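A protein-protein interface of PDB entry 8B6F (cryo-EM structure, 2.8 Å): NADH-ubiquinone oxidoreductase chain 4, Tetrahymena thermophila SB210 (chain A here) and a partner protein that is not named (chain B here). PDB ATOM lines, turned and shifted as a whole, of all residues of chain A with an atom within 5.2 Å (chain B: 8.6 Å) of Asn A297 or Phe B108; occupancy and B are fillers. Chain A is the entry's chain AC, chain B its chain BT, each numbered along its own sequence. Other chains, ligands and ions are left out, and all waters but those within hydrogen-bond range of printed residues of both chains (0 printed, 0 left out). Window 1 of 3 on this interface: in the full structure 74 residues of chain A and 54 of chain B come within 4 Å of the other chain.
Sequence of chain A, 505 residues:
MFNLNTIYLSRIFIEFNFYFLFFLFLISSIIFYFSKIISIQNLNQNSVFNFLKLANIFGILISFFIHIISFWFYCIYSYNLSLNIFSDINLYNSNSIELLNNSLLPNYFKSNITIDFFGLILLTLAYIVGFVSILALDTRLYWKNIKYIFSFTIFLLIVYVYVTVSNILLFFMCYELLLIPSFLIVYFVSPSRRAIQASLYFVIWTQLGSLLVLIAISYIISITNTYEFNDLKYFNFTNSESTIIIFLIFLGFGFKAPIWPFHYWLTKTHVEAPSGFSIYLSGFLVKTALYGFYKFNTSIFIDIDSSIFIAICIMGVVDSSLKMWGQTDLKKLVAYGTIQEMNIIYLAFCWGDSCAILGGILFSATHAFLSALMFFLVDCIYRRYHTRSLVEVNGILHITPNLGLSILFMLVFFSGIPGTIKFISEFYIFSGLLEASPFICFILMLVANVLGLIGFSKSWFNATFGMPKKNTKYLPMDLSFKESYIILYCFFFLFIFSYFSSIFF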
ATOM      1  N   ILE A 246     -29.620   7.846 -14.285  1.00  0.00           N
ATOM      2  CA  ILE A 246     -29.132   9.022 -13.571  1.00  0.00           C
ATOM      3  C   ILE A 246     -30.028  10.225 -13.843  1.00  0.00           C
ATOM      4  O   ILE A 246     -30.341  10.995 -12.928  1.00  0.00           O
ATOM      5  CB  ILE A 246     -27.661   9.311 -13.924  1.00  0.00           C
ATOM      6  CG1 ILE A 246     -27.140  10.524 -13.142  1.00  0.00           C
ATOM      7  CG2 ILE A 246     -27.501   9.576 -15.404  1.00  0.00           C
ATOM      8  CD1 ILE A 246     -27.328  10.446 -11.636  1.00  0.00           C
ATOM      9  N   GLY A 292     -31.599   9.510  -0.719  1.00  0.00           N
ATOM     10  CA  GLY A 292     -31.907   8.515  -1.732  1.00  0.00           C
ATOM     11  C   GLY A 292     -31.098   8.704  -3.000  1.00  0.00           C
ATOM     12  O   GLY A 292     -30.622   7.733  -3.593  1.00  0.00           O
ATOM     13  N   PHE A 293     -30.937   9.954  -3.439  1.00  0.00           N
ATOM     14  CA  PHE A 293     -30.113  10.221  -4.613  1.00  0.00           C
ATOM     15  C   PHE A 293     -28.680   9.764  -4.387  1.00  0.00           C
ATOM     16  O   PHE A 293     -28.073   9.138  -5.262  1.00  0.00           O
ATOM     17  CB  PHE A 293     -30.150  11.711  -4.955  1.00  0.00           C
ATOM     18  CG  PHE A 293     -29.145  12.117  -5.995  1.00  0.00           C
ATOM     19  CD1 PHE A 293     -29.461  12.056  -7.339  1.00  0.00           C
ATOM     20  CD2 PHE A 293     -27.889  12.569  -5.628  1.00  0.00           C
ATOM     21  CE1 PHE A 293     -28.542  12.429  -8.299  1.00  0.00           C
ATOM     22  CE2 PHE A 293     -26.965  12.944  -6.583  1.00  0.00           C
ATOM     23  CZ  PHE A 293     -27.293  12.874  -7.920  1.00  0.00           C
ATOM     24  N   TYR A 294     -28.121  10.072  -3.217  1.00  0.00           N
ATOM     25  CA  TYR A 294     -26.771   9.625  -2.897  1.00  0.00           C
ATOM     26  C   TYR A 294     -26.663   8.109  -2.977  1.00  0.00           C
ATOM     27  O   TYR A 294     -25.758   7.572  -3.625  1.00  0.00           O
ATOM     28  CB  TYR A 294     -26.382  10.122  -1.505  1.00  0.00           C
ATOM     29  CG  TYR A 294     -25.231   9.368  -0.886  1.00  0.00           C
ATOM     30  CD1 TYR A 294     -23.918   9.690  -1.196  1.00  0.00           C
ATOM     31  CD2 TYR A 294     -25.460   8.337   0.013  1.00  0.00           C
ATOM     32  CE1 TYR A 294     -22.865   9.004  -0.631  1.00  0.00           C
ATOM     33  CE2 TYR A 294     -24.414   7.646   0.585  1.00  0.00           C
ATOM     34  CZ  TYR A 294     -23.119   7.984   0.258  1.00  0.00           C
ATOM     35  OH  TYR A 294     -22.074   7.296   0.826  1.00  0.00           O
ATOM     36  N   LYS A 295     -27.575   7.398  -2.316  1.00  0.00           N
ATOM     37  CA  LYS A 295     -27.509   5.940  -2.314  1.00  0.00           C
ATOM     38  C   LYS A 295     -27.548   5.387  -3.733  1.00  0.00           C
ATOM     39  O   LYS A 295     -26.703   4.572  -4.117  1.00  0.00           O
ATOM     40  CB  LYS A 295     -28.657   5.369  -1.483  1.00  0.00           C
ATOM     41  CG  LYS A 295     -28.601   5.743  -0.009  1.00  0.00           C
ATOM     42  CD  LYS A 295     -27.516   4.981   0.736  1.00  0.00           C
ATOM     43  CE  LYS A 295     -27.900   3.532   0.986  1.00  0.00           C
ATOM     44  NZ  LYS A 295     -29.136   3.397   1.802  1.00  0.00           N
ATOM     45  N   PHE A 296     -28.533   5.811  -4.526  1.00  0.00           N
ATOM     46  CA  PHE A 296     -28.704   5.239  -5.858  1.00  0.00           C
ATOM     47  C   PHE A 296     -27.528   5.567  -6.769  1.00  0.00           C
ATOM     48  O   PHE A 296     -27.025   4.688  -7.478  1.00  0.00           O
ATOM     49  CB  PHE A 296     -30.012   5.739  -6.476  1.00  0.00           C
ATOM     50  CG  PHE A 296     -31.239   5.192  -5.808  1.00  0.00           C
ATOM     51  CD1 PHE A 296     -31.296   3.871  -5.398  1.00  0.00           C
ATOM     52  CD2 PHE A 296     -32.329   6.008  -5.573  1.00  0.00           C
ATOM     53  CE1 PHE A 296     -32.421   3.371  -4.781  1.00  0.00           C
ATOM     54  CE2 PHE A 296     -33.456   5.514  -4.954  1.00  0.00           C
ATOM     55  CZ  PHE A 296     -33.499   4.196  -4.550  1.00  0.00           C
ATOM     56  N   ASN A 297     -27.073   6.821  -6.769  1.00  0.00           N
ATOM     57  CA  ASN A 297     -26.024   7.212  -7.704  1.00  0.00           C
ATOM     58  C   ASN A 297     -24.666   6.650  -7.305  1.00  0.00           C
ATOM     59  O   ASN A 297     -23.821   6.412  -8.175  1.00  0.00           O
ATOM     60  CB  ASN A 297     -25.957   8.737  -7.826  1.00  0.00           C
ATOM     61  CG  ASN A 297     -25.089   9.373  -6.764  1.00  0.00           C
ATOM     62  OD1 ASN A 297     -25.083   8.945  -5.614  1.00  0.00           O
ATOM     63  ND2 ASN A 297     -24.342  10.400  -7.149  1.00  0.00           N
ATOM     64  N   THR A 298     -24.429   6.432  -6.010  1.00  0.00           N
ATOM     65  CA  THR A 298     -23.191   5.781  -5.599  1.00  0.00           C
ATOM     66  C   THR A 298     -23.225   4.275  -5.829  1.00  0.00           C
ATOM     67  O   THR A 298     -22.168   3.655  -5.983  1.00  0.00           O
ATOM     68  CB  THR A 298     -22.906   6.071  -4.124  1.00  0.00           C
ATOM     69  OG1 THR A 298     -24.038   5.699  -3.330  1.00  0.00           O
ATOM     70  CG2 THR A 298     -22.612   7.543  -3.920  1.00  0.00           C
ATOM     71  N   SER A 299     -24.412   3.669  -5.839  1.00  0.00           N
ATOM     72  CA  SER A 299     -24.518   2.251  -6.159  1.00  0.00           C
ATOM     73  C   SER A 299     -24.373   1.989  -7.653  1.00  0.00           C
ATOM     74  O   SER A 299     -23.780   0.980  -8.051  1.00  0.00           O
ATOM     75  CB  SER A 299     -25.837   1.692  -5.638  1.00  0.00           C
ATOM     76  OG  SER A 299     -25.841   1.743  -4.226  1.00  0.00           O
ATOM     77  N   ILE A 300     -24.897   2.870  -8.485  1.00  0.00           N
ATOM     78  CA  ILE A 300     -24.827   2.700  -9.930  1.00  0.00           C
ATOM     79  C   ILE A 300     -23.544   3.339 -10.431  1.00  0.00           C
ATOM     80  O   ILE A 300     -23.070   4.346  -9.895  1.00  0.00           O
ATOM     81  CB  ILE A 300     -26.066   3.314 -10.619  1.00  0.00           C
ATOM     82  CG1 ILE A 300     -27.359   2.689 -10.082  1.00  0.00           C
ATOM     83  CG2 ILE A 300     -25.979   3.156 -12.134  1.00  0.00           C
ATOM     84  CD1 ILE A 300     -27.500   1.209 -10.356  1.00  0.00           C
ATOM     85  N   PHE A 301     -22.974   2.745 -11.474  1.00  0.00           N
ATOM     86  CA  PHE A 301     -21.809   3.298 -12.148  1.00  0.00           C
ATOM     87  C   PHE A 301     -22.283   4.155 -13.313  1.00  0.00           C
ATOM     88  O   PHE A 301     -22.996   3.670 -14.198  1.00  0.00           O
ATOM     89  CB  PHE A 301     -20.884   2.188 -12.638  1.00  0.00           C
ATOM     90  CG  PHE A 301     -19.766   2.679 -13.510  1.00  0.00           C
ATOM     91  CD1 PHE A 301     -18.591   3.152 -12.950  1.00  0.00           C
ATOM     92  CD2 PHE A 301     -19.889   2.664 -14.889  1.00  0.00           C
ATOM     93  CE1 PHE A 301     -17.561   3.605 -13.750  1.00  0.00           C
ATOM     94  CE2 PHE A 301     -18.862   3.116 -15.696  1.00  0.00           C
ATOM     95  CZ  PHE A 301     -17.697   3.588 -15.125  1.00  0.00           C
ATOM     96  N   ILE A 302     -21.883   5.421 -13.316  1.00  0.00           N
ATOM     97  CA  ILE A 302     -22.341   6.394 -14.297  1.00  0.00           C
ATOM     98  C   ILE A 302     -21.124   6.932 -15.033  1.00  0.00           C
ATOM     99  O   ILE A 302     -20.151   7.361 -14.402  1.00  0.00           O
ATOM    100  CB  ILE A 302     -23.131   7.534 -13.635  1.00  0.00           C
ATOM    101  CG1 ILE A 302     -24.126   6.974 -12.613  1.00  0.00           C
ATOM    102  CG2 ILE A 302     -23.870   8.310 -14.689  1.00  0.00           C
ATOM    103  CD1 ILE A 302     -24.800   8.029 -11.779  1.00  0.00           C
ATOM    104  N   ILE A 304     -21.218   9.496 -17.449  1.00  0.00           N
ATOM    105  CA  ILE A 304     -21.734  10.667 -18.143  1.00  0.00           C
ATOM    106  C   ILE A 304     -21.159  11.912 -17.483  1.00  0.00           C
ATOM    107  O   ILE A 304     -20.754  11.902 -16.319  1.00  0.00           O
ATOM    108  CB  ILE A 304     -23.279  10.710 -18.134  1.00  0.00           C
ATOM    109  CG1 ILE A 304     -23.788  11.714 -19.170  1.00  0.00           C
ATOM    110  CG2 ILE A 304     -23.799  11.121 -16.757  1.00  0.00           C
ATOM    111  CD1 ILE A 304     -25.299  11.783 -19.282  1.00  0.00           C
ATOM    112  N   ASP A 305     -21.123  12.995 -18.252  1.00  0.00           N
ATOM    113  CA  ASP A 305     -20.681  14.276 -17.723  1.00  0.00           C
ATOM    114  C   ASP A 305     -21.769  14.868 -16.837  1.00  0.00           C
ATOM    115  O   ASP A 305     -22.932  14.958 -17.242  1.00  0.00           O
ATOM    116  CB  ASP A 305     -20.349  15.229 -18.871  1.00  0.00           C
ATOM    117  CG  ASP A 305     -19.808  16.561 -18.390  1.00  0.00           C
ATOM    118  OD1 ASP A 305     -19.606  16.721 -17.169  1.00  0.00           O
ATOM    119  OD2 ASP A 305     -19.586  17.453 -19.235  1.00  0.00           O
ATOM    120  N   SER A 306     -21.392  15.274 -15.627  1.00  0.00           N
ATOM    121  CA  SER A 306     -22.325  15.862 -14.677  1.00  0.00           C
ATOM    122  C   SER A 306     -22.439  17.372 -14.829  1.00  0.00           C
ATOM    123  O   SER A 306     -22.989  18.032 -13.943  1.00  0.00           O
ATOM    124  CB  SER A 306     -21.912  15.514 -13.244  1.00  0.00           C
ATOM    125  OG  SER A 306     -20.651  16.067 -12.919  1.00  0.00           O
ATOM    126  N   PHE A 309     -26.094  18.656 -14.655  1.00  0.00           N
ATOM    127  CA  PHE A 309     -26.665  18.670 -13.311  1.00  0.00           C
ATOM    128  C   PHE A 309     -26.052  19.780 -12.470  1.00  0.00           C
ATOM    129  O   PHE A 309     -26.760  20.462 -11.721  1.00  0.00           O
ATOM    130  CB  PHE A 309     -26.467  17.308 -12.648  1.00  0.00           C
ATOM    131  CG  PHE A 309     -26.894  16.155 -13.506  1.00  0.00           C
ATOM    132  CD1 PHE A 309     -28.223  16.006 -13.872  1.00  0.00           C
ATOM    133  CD2 PHE A 309     -25.974  15.220 -13.942  1.00  0.00           C
ATOM    134  CE1 PHE A 309     -28.623  14.947 -14.660  1.00  0.00           C
ATOM    135  CE2 PHE A 309     -26.368  14.158 -14.731  1.00  0.00           C
ATOM    136  CZ  PHE A 309     -27.695  14.021 -15.092  1.00  0.00           C
ATOM    137  N   PHE A 349     -23.429  16.724  -4.304  1.00  0.00           N
ATOM    138  CA  PHE A 349     -23.556  15.305  -4.611  1.00  0.00           C
ATOM    139  C   PHE A 349     -23.403  15.008  -6.101  1.00  0.00           C
ATOM    140  O   PHE A 349     -23.789  13.927  -6.554  1.00  0.00           O
ATOM    141  CB  PHE A 349     -24.907  14.782  -4.118  1.00  0.00           C
ATOM    142  CG  PHE A 349     -25.001  14.650  -2.626  1.00  0.00           C
ATOM    143  CD1 PHE A 349     -25.457  15.703  -1.853  1.00  0.00           C
ATOM    144  CD2 PHE A 349     -24.642  13.472  -1.997  1.00  0.00           C
ATOM    145  CE1 PHE A 349     -25.547  15.587  -0.482  1.00  0.00           C
ATOM    146  CE2 PHE A 349     -24.731  13.349  -0.624  1.00  0.00           C
ATOM    147  CZ  PHE A 349     -25.184  14.408   0.133  1.00  0.00           C
ATOM    148  N   CYS A 350     -22.848  15.937  -6.873  1.00  0.00           N
ATOM    149  CA  CYS A 350     -22.771  15.781  -8.319  1.00  0.00           C
ATOM    150  C   CYS A 350     -21.482  15.120  -8.791  1.00  0.00           C
ATOM    151  O   CYS A 350     -21.280  14.995 -10.002  1.00  0.00           O
ATOM    152  CB  CYS A 350     -22.919  17.145  -9.000  1.00  0.00           C
ATOM    153  SG  CYS A 350     -24.593  17.810  -8.945  1.00  0.00           S
ATOM    154  N   TRP A 351     -20.609  14.697  -7.880  1.00  0.00           N
ATOM    155  CA  TRP A 351     -19.358  14.034  -8.227  1.00  0.00           C
ATOM    156  C   TRP A 351     -19.330  12.609  -7.689  1.00  0.00           C
ATOM    157  O   TRP A 351     -18.312  12.138  -7.179  1.00  0.00           O
ATOM    158  CB  TRP A 351     -18.159  14.826  -7.709  1.00  0.00           C
ATOM    159  CG  TRP A 351     -17.895  16.080  -8.480  1.00  0.00           C
ATOM    160  CD1 TRP A 351     -17.075  16.218  -9.559  1.00  0.00           C
ATOM    161  CD2 TRP A 351     -18.457  17.372  -8.233  1.00  0.00           C
ATOM    162  NE1 TRP A 351     -17.091  17.519 -10.001  1.00  0.00           N
ATOM    163  CE2 TRP A 351     -17.932  18.247  -9.202  1.00  0.00           C
ATOM    164  CE3 TRP A 351     -19.354  17.874  -7.284  1.00  0.00           C
ATOM    165  CZ2 TRP A 351     -18.273  19.595  -9.252  1.00  0.00           C
ATOM    166  CZ3 TRP A 351     -19.691  19.213  -7.334  1.00  0.00           C
ATOM    167  CH2 TRP A 351     -19.152  20.058  -8.312  1.00  0.00           C
ATOM    168  N   GLY A 352     -20.451  11.908  -7.799  1.00  0.00           N
ATOM    169  CA  GLY A 352     -20.497  10.530  -7.341  1.00  0.00           C
ATOM    170  C   GLY A 352     -20.191  10.433  -5.861  1.00  0.00           C
ATOM    171  O   GLY A 352     -20.728  11.183  -5.039  1.00  0.00           O
ATOM    172  N   SER B 105     -12.539  16.331 -12.753  1.00  0.00           N
ATOM    173  CA  SER B 105     -13.453  16.488 -13.870  1.00  0.00           C
ATOM    174  C   SER B 105     -14.881  16.262 -13.393  1.00  0.00           C
ATOM    175  O   SER B 105     -15.122  15.612 -12.374  1.00  0.00           O
ATOM    176  CB  SER B 105     -13.118  15.505 -14.998  1.00  0.00           C
ATOM    177  OG  SER B 105     -13.968  15.700 -16.114  1.00  0.00           O
ATOM    178  N   ASN B 106     -15.833  16.814 -14.142  1.00  0.00           N
ATOM    179  CA  ASN B 106     -17.254  16.697 -13.813  1.00  0.00           C
ATOM    180  C   ASN B 106     -17.734  15.302 -14.194  1.00  0.00           C
ATOM    181  O   ASN B 106     -18.201  15.065 -15.309  1.00  0.00           O
ATOM    182  CB  ASN B 106     -18.062  17.778 -14.518  1.00  0.00           C
ATOM    183  CG  ASN B 106     -17.748  19.167 -14.004  1.00  0.00           C
ATOM    184  OD1 ASN B 106     -17.264  19.331 -12.886  1.00  0.00           O
ATOM    185  ND2 ASN B 106     -18.028  20.175 -14.816  1.00  0.00           N
ATOM    186  N   LYS B 107     -17.619  14.361 -13.259  1.00  0.00           N
ATOM    187  CA  LYS B 107     -18.076  12.999 -13.491  1.00  0.00           C
ATOM    188  C   LYS B 107     -18.445  12.358 -12.163  1.00  0.00           C
ATOM    189  O   LYS B 107     -18.016  12.803 -11.096  1.00  0.00           O
ATOM    190  CB  LYS B 107     -17.009  12.160 -14.207  1.00  0.00           C
ATOM    191  CG  LYS B 107     -16.815  12.532 -15.668  1.00  0.00           C
ATOM    192  CD  LYS B 107     -15.956  11.510 -16.395  1.00  0.00           C
ATOM    193  CE  LYS B 107     -15.952  11.761 -17.893  1.00  0.00           C
ATOM    194  NZ  LYS B 107     -15.437  13.117 -18.235  1.00  0.00           N
ATOM    195  N   PHE B 108     -19.257  11.304 -12.243  1.00  0.00           N
ATOM    196  CA  PHE B 108     -19.665  10.539 -11.064  1.00  0.00           C
ATOM    197  C   PHE B 108     -18.593   9.493 -10.789  1.00  0.00           C
ATOM    198  O   PHE B 108     -18.663   8.359 -11.261  1.00  0.00           O
ATOM    199  CB  PHE B 108     -21.031   9.895 -11.276  1.00  0.00           C
ATOM    200  CG  PHE B 108     -22.139  10.881 -11.493  1.00  0.00           C
ATOM    201  CD1 PHE B 108     -22.431  11.346 -12.764  1.00  0.00           C
ATOM    202  CD2 PHE B 108     -22.890  11.345 -10.426  1.00  0.00           C
ATOM    203  CE1 PHE B 108     -23.450  12.256 -12.966  1.00  0.00           C
ATOM    204  CE2 PHE B 108     -23.911  12.254 -10.622  1.00  0.00           C
ATOM    205  CZ  PHE B 108     -24.191  12.709 -11.893  1.00  0.00           C
ATOM    206  N   TYR B 109     -17.584   9.883 -10.016  1.00  0.00           N
ATOM    207  CA  TYR B 109     -16.502   8.967  -9.691  1.00  0.00           C
ATOM    208  C   TYR B 109     -17.028   7.777  -8.901  1.00  0.00           C
ATOM    209  O   TYR B 109     -17.956   7.897  -8.097  1.00  0.00           O
ATOM    210  CB  TYR B 109     -15.416   9.681  -8.895  1.00  0.00           C
ATOM    211  CG  TYR B 109     -14.692  10.719  -9.703  1.00  0.00           C
ATOM    212  CD1 TYR B 109     -13.724  10.353 -10.629  1.00  0.00           C
ATOM    213  CD2 TYR B 109     -14.975  12.064  -9.544  1.00  0.00           C
ATOM    214  CE1 TYR B 109     -13.063  11.297 -11.370  1.00  0.00           C
ATOM    215  CE2 TYR B 109     -14.320  13.012 -10.278  1.00  0.00           C
ATOM    216  CZ  TYR B 109     -13.366  12.623 -11.187  1.00  0.00           C
ATOM    217  OH  TYR B 109     -12.732  13.592 -11.904  1.00  0.00           O
ATOM    218  N   HIS B 110     -16.428   6.617  -9.142  1.00  0.00           N
ATOM    219  CA  HIS B 110     -16.893   5.353  -8.586  1.00  0.00           C
ATOM    220  C   HIS B 110     -15.736   4.603  -7.941  1.00  0.00           C
ATOM    221  O   HIS B 110     -15.521   3.412  -8.179  1.00  0.00           O
ATOM    222  CB  HIS B 110     -17.560   4.514  -9.670  1.00  0.00           C
ATOM    223  CG  HIS B 110     -18.478   3.463  -9.134  1.00  0.00           C
ATOM    224  ND1 HIS B 110     -18.058   2.182  -8.845  1.00  0.00           N
ATOM    225  CD2 HIS B 110     -19.796   3.504  -8.826  1.00  0.00           C
ATOM    226  CE1 HIS B 110     -19.077   1.479  -8.388  1.00  0.00           C
ATOM    227  NE2 HIS B 110     -20.143   2.257  -8.365  1.00  0.00           N
ATOM    228  N   ASN B 111     -14.961   5.304  -7.110  1.00  0.00           N
ATOM    229  CA  ASN B 111     -13.835   4.662  -6.439  1.00  0.00           C
ATOM    230  C   ASN B 111     -14.309   3.521  -5.552  1.00  0.00           C
ATOM    231  O   ASN B 111     -13.715   2.437  -5.545  1.00  0.00           O
ATOM    232  CB  ASN B 111     -13.055   5.679  -5.605  1.00  0.00           C
ATOM    233  CG  ASN B 111     -12.948   7.028  -6.278  1.00  0.00           C
ATOM    234  OD1 ASN B 111     -12.486   7.136  -7.413  1.00  0.00           O
ATOM    235  ND2 ASN B 111     -13.389   8.066  -5.581  1.00  0.00           N
ATOM    236  N   ASN B 112     -15.371   3.753  -4.787  1.00  0.00           N
ATOM    237  CA  ASN B 112     -15.950   2.714  -3.950  1.00  0.00           C
ATOM    238  C   ASN B 112     -16.870   1.835  -4.785  1.00  0.00           C
ATOM    239  O   ASN B 112     -17.745   2.337  -5.496  1.00  0.00           O
ATOM    240  CB  ASN B 112     -16.727   3.336  -2.793  1.00  0.00           C
ATOM    241  CG  ASN B 112     -15.986   4.483  -2.141  1.00  0.00           C
ATOM    242  OD1 ASN B 112     -14.997   4.982  -2.675  1.00  0.00           O
ATOM    243  ND2 ASN B 112     -16.466   4.914  -0.981  1.00  0.00           N
ATOM    244  N   GLY B 114     -19.569   0.526  -4.747  1.00  0.00           N
ATOM    245  CA  GLY B 114     -20.873   0.537  -4.124  1.00  0.00           C
ATOM    246  C   GLY B 114     -20.830   0.510  -2.615  1.00  0.00           C
ATOM    247  O   GLY B 114     -21.878   0.349  -1.982  1.00  0.00           O
ATOM    248  N   PHE B 116     -20.884   2.154   0.713  1.00  0.00           N
ATOM    249  CA  PHE B 116     -21.317   3.447   1.213  1.00  0.00           C
ATOM    250  C   PHE B 116     -20.392   3.935   2.324  1.00  0.00           C
ATOM    251  O   PHE B 116     -19.646   3.168   2.938  1.00  0.00           O
ATOM    252  CB  PHE B 116     -22.756   3.362   1.720  1.00  0.00           C
ATOM    253  CG  PHE B 116     -23.743   2.958   0.665  1.00  0.00           C
ATOM    254  CD1 PHE B 116     -23.755   3.586  -0.571  1.00  0.00           C
ATOM    255  CD2 PHE B 116     -24.646   1.937   0.900  1.00  0.00           C
ATOM    256  CE1 PHE B 116     -24.655   3.209  -1.546  1.00  0.00           C
ATOM    257  CE2 PHE B 116     -25.548   1.556  -0.071  1.00  0.00           C
ATOM    258  CZ  PHE B 116     -25.553   2.193  -1.296  1.00  0.00           C
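The backbone carbonyl oxygen (O) of Asn B106 sits at hydrogen-bond distance from the backbone NH (N) of Ser A306, at 3.2 Å. O of Thr A298 is in hydrogen-bond range of NE2 of His B110 (3.4 Å). The indole nitrogen (NE1) of Trp A351 lies within hydrogen-bond range of the side-chain amide oxygen (OD1) of Asn B106. The side-chain carboxylate of Asp A305 lies close to the backbone carbonyl oxygen of Asn B106 (2.9 Å). N of Lys B107 lies within hydrogen-bond range of OG of Ser A306, 3.5 Å away.
A ring nitrogen (ND1) of His B110 lies close to the backbone carbonyl oxygen of Asn B112 (3.4 Å). The backbone NH (N) of Ser B105 is in hydrogen-bond range of the side-chain hydroxyl (OH) of Tyr B109, at 2.9 Å. The backbone carbonyl oxygen (O) of Lys A295 sits at hydrogen-bond distance from the side-chain hydroxyl (OG) of Ser A299 (3.0 Å). The side-chain hydroxyl of Thr A298 sits at hydrogen-bond distance from the backbone carbonyl oxygen of Lys A295, at 3.0 Å. OG1 of Thr A298 lies within hydrogen-bond range of O of Tyr A294 (2.6 Å). O of Phe A293 sits close to OD1 of Asn A297 (3.0 Å).
Tyr A294 touches Phe B116 (OH to CA, 3.9 Å). Phe B108 touches Asn A297. Thr A298 touches Phe B116 (OG1 to CE1, 3.1 Å). Ser A299 touches Phe B116. Phe A301 touches His B110 (CD1 to CB, 3.7 Å). Phe B108 touches Ile A304. Phe B108 touches Ser A306 (CE1 to CB, 3.6 Å). Phe A309 touches Phe B108 (CD2 to CZ, 3.7 Å). CD1 of Trp A351 touches O of Ser B105 (3.5 Å). N of Gly A352 touches CA of Phe B108 (3.6 Å).
Phe A293 touches none of the printed residues of chain B. Printed residues of chain B within 4 Å of Tyr A294: Phe B116 (3.9 Å). Of chain B, only Phe B108 (3.7 Å) comes within 4 Å of Asn A297. Printed residues of chain B within 4 Å of Asp A305: Asn B106. Phe A349 touches none of the printed residues of chain B. Phe B108 touches just these residues of chain A: Ile A246, Asn A297, Ile A302, Ile A304, Ser A306, Phe A309, Cys A350, Trp A351 and Gly A352. The nearest printed residue of chain A that does not touch Phe B108 is Phe A293 (4.4 Å).
Printed residues of chain A that touch a printed residue of chain B: Ile A246, Tyr A294, Lys A295, Asn A297, Thr A298, Ser A299, Ile A300, Phe A301, Ile A302, Ile A304, Asp A305, Ser A306, Phe A309, Cys A350, Trp A351 and Gly A352. Hydrophobic or aromatic side chains of chain B within 4 Å of the printed part of chain A: Phe B108, His B110 and Phe B116.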
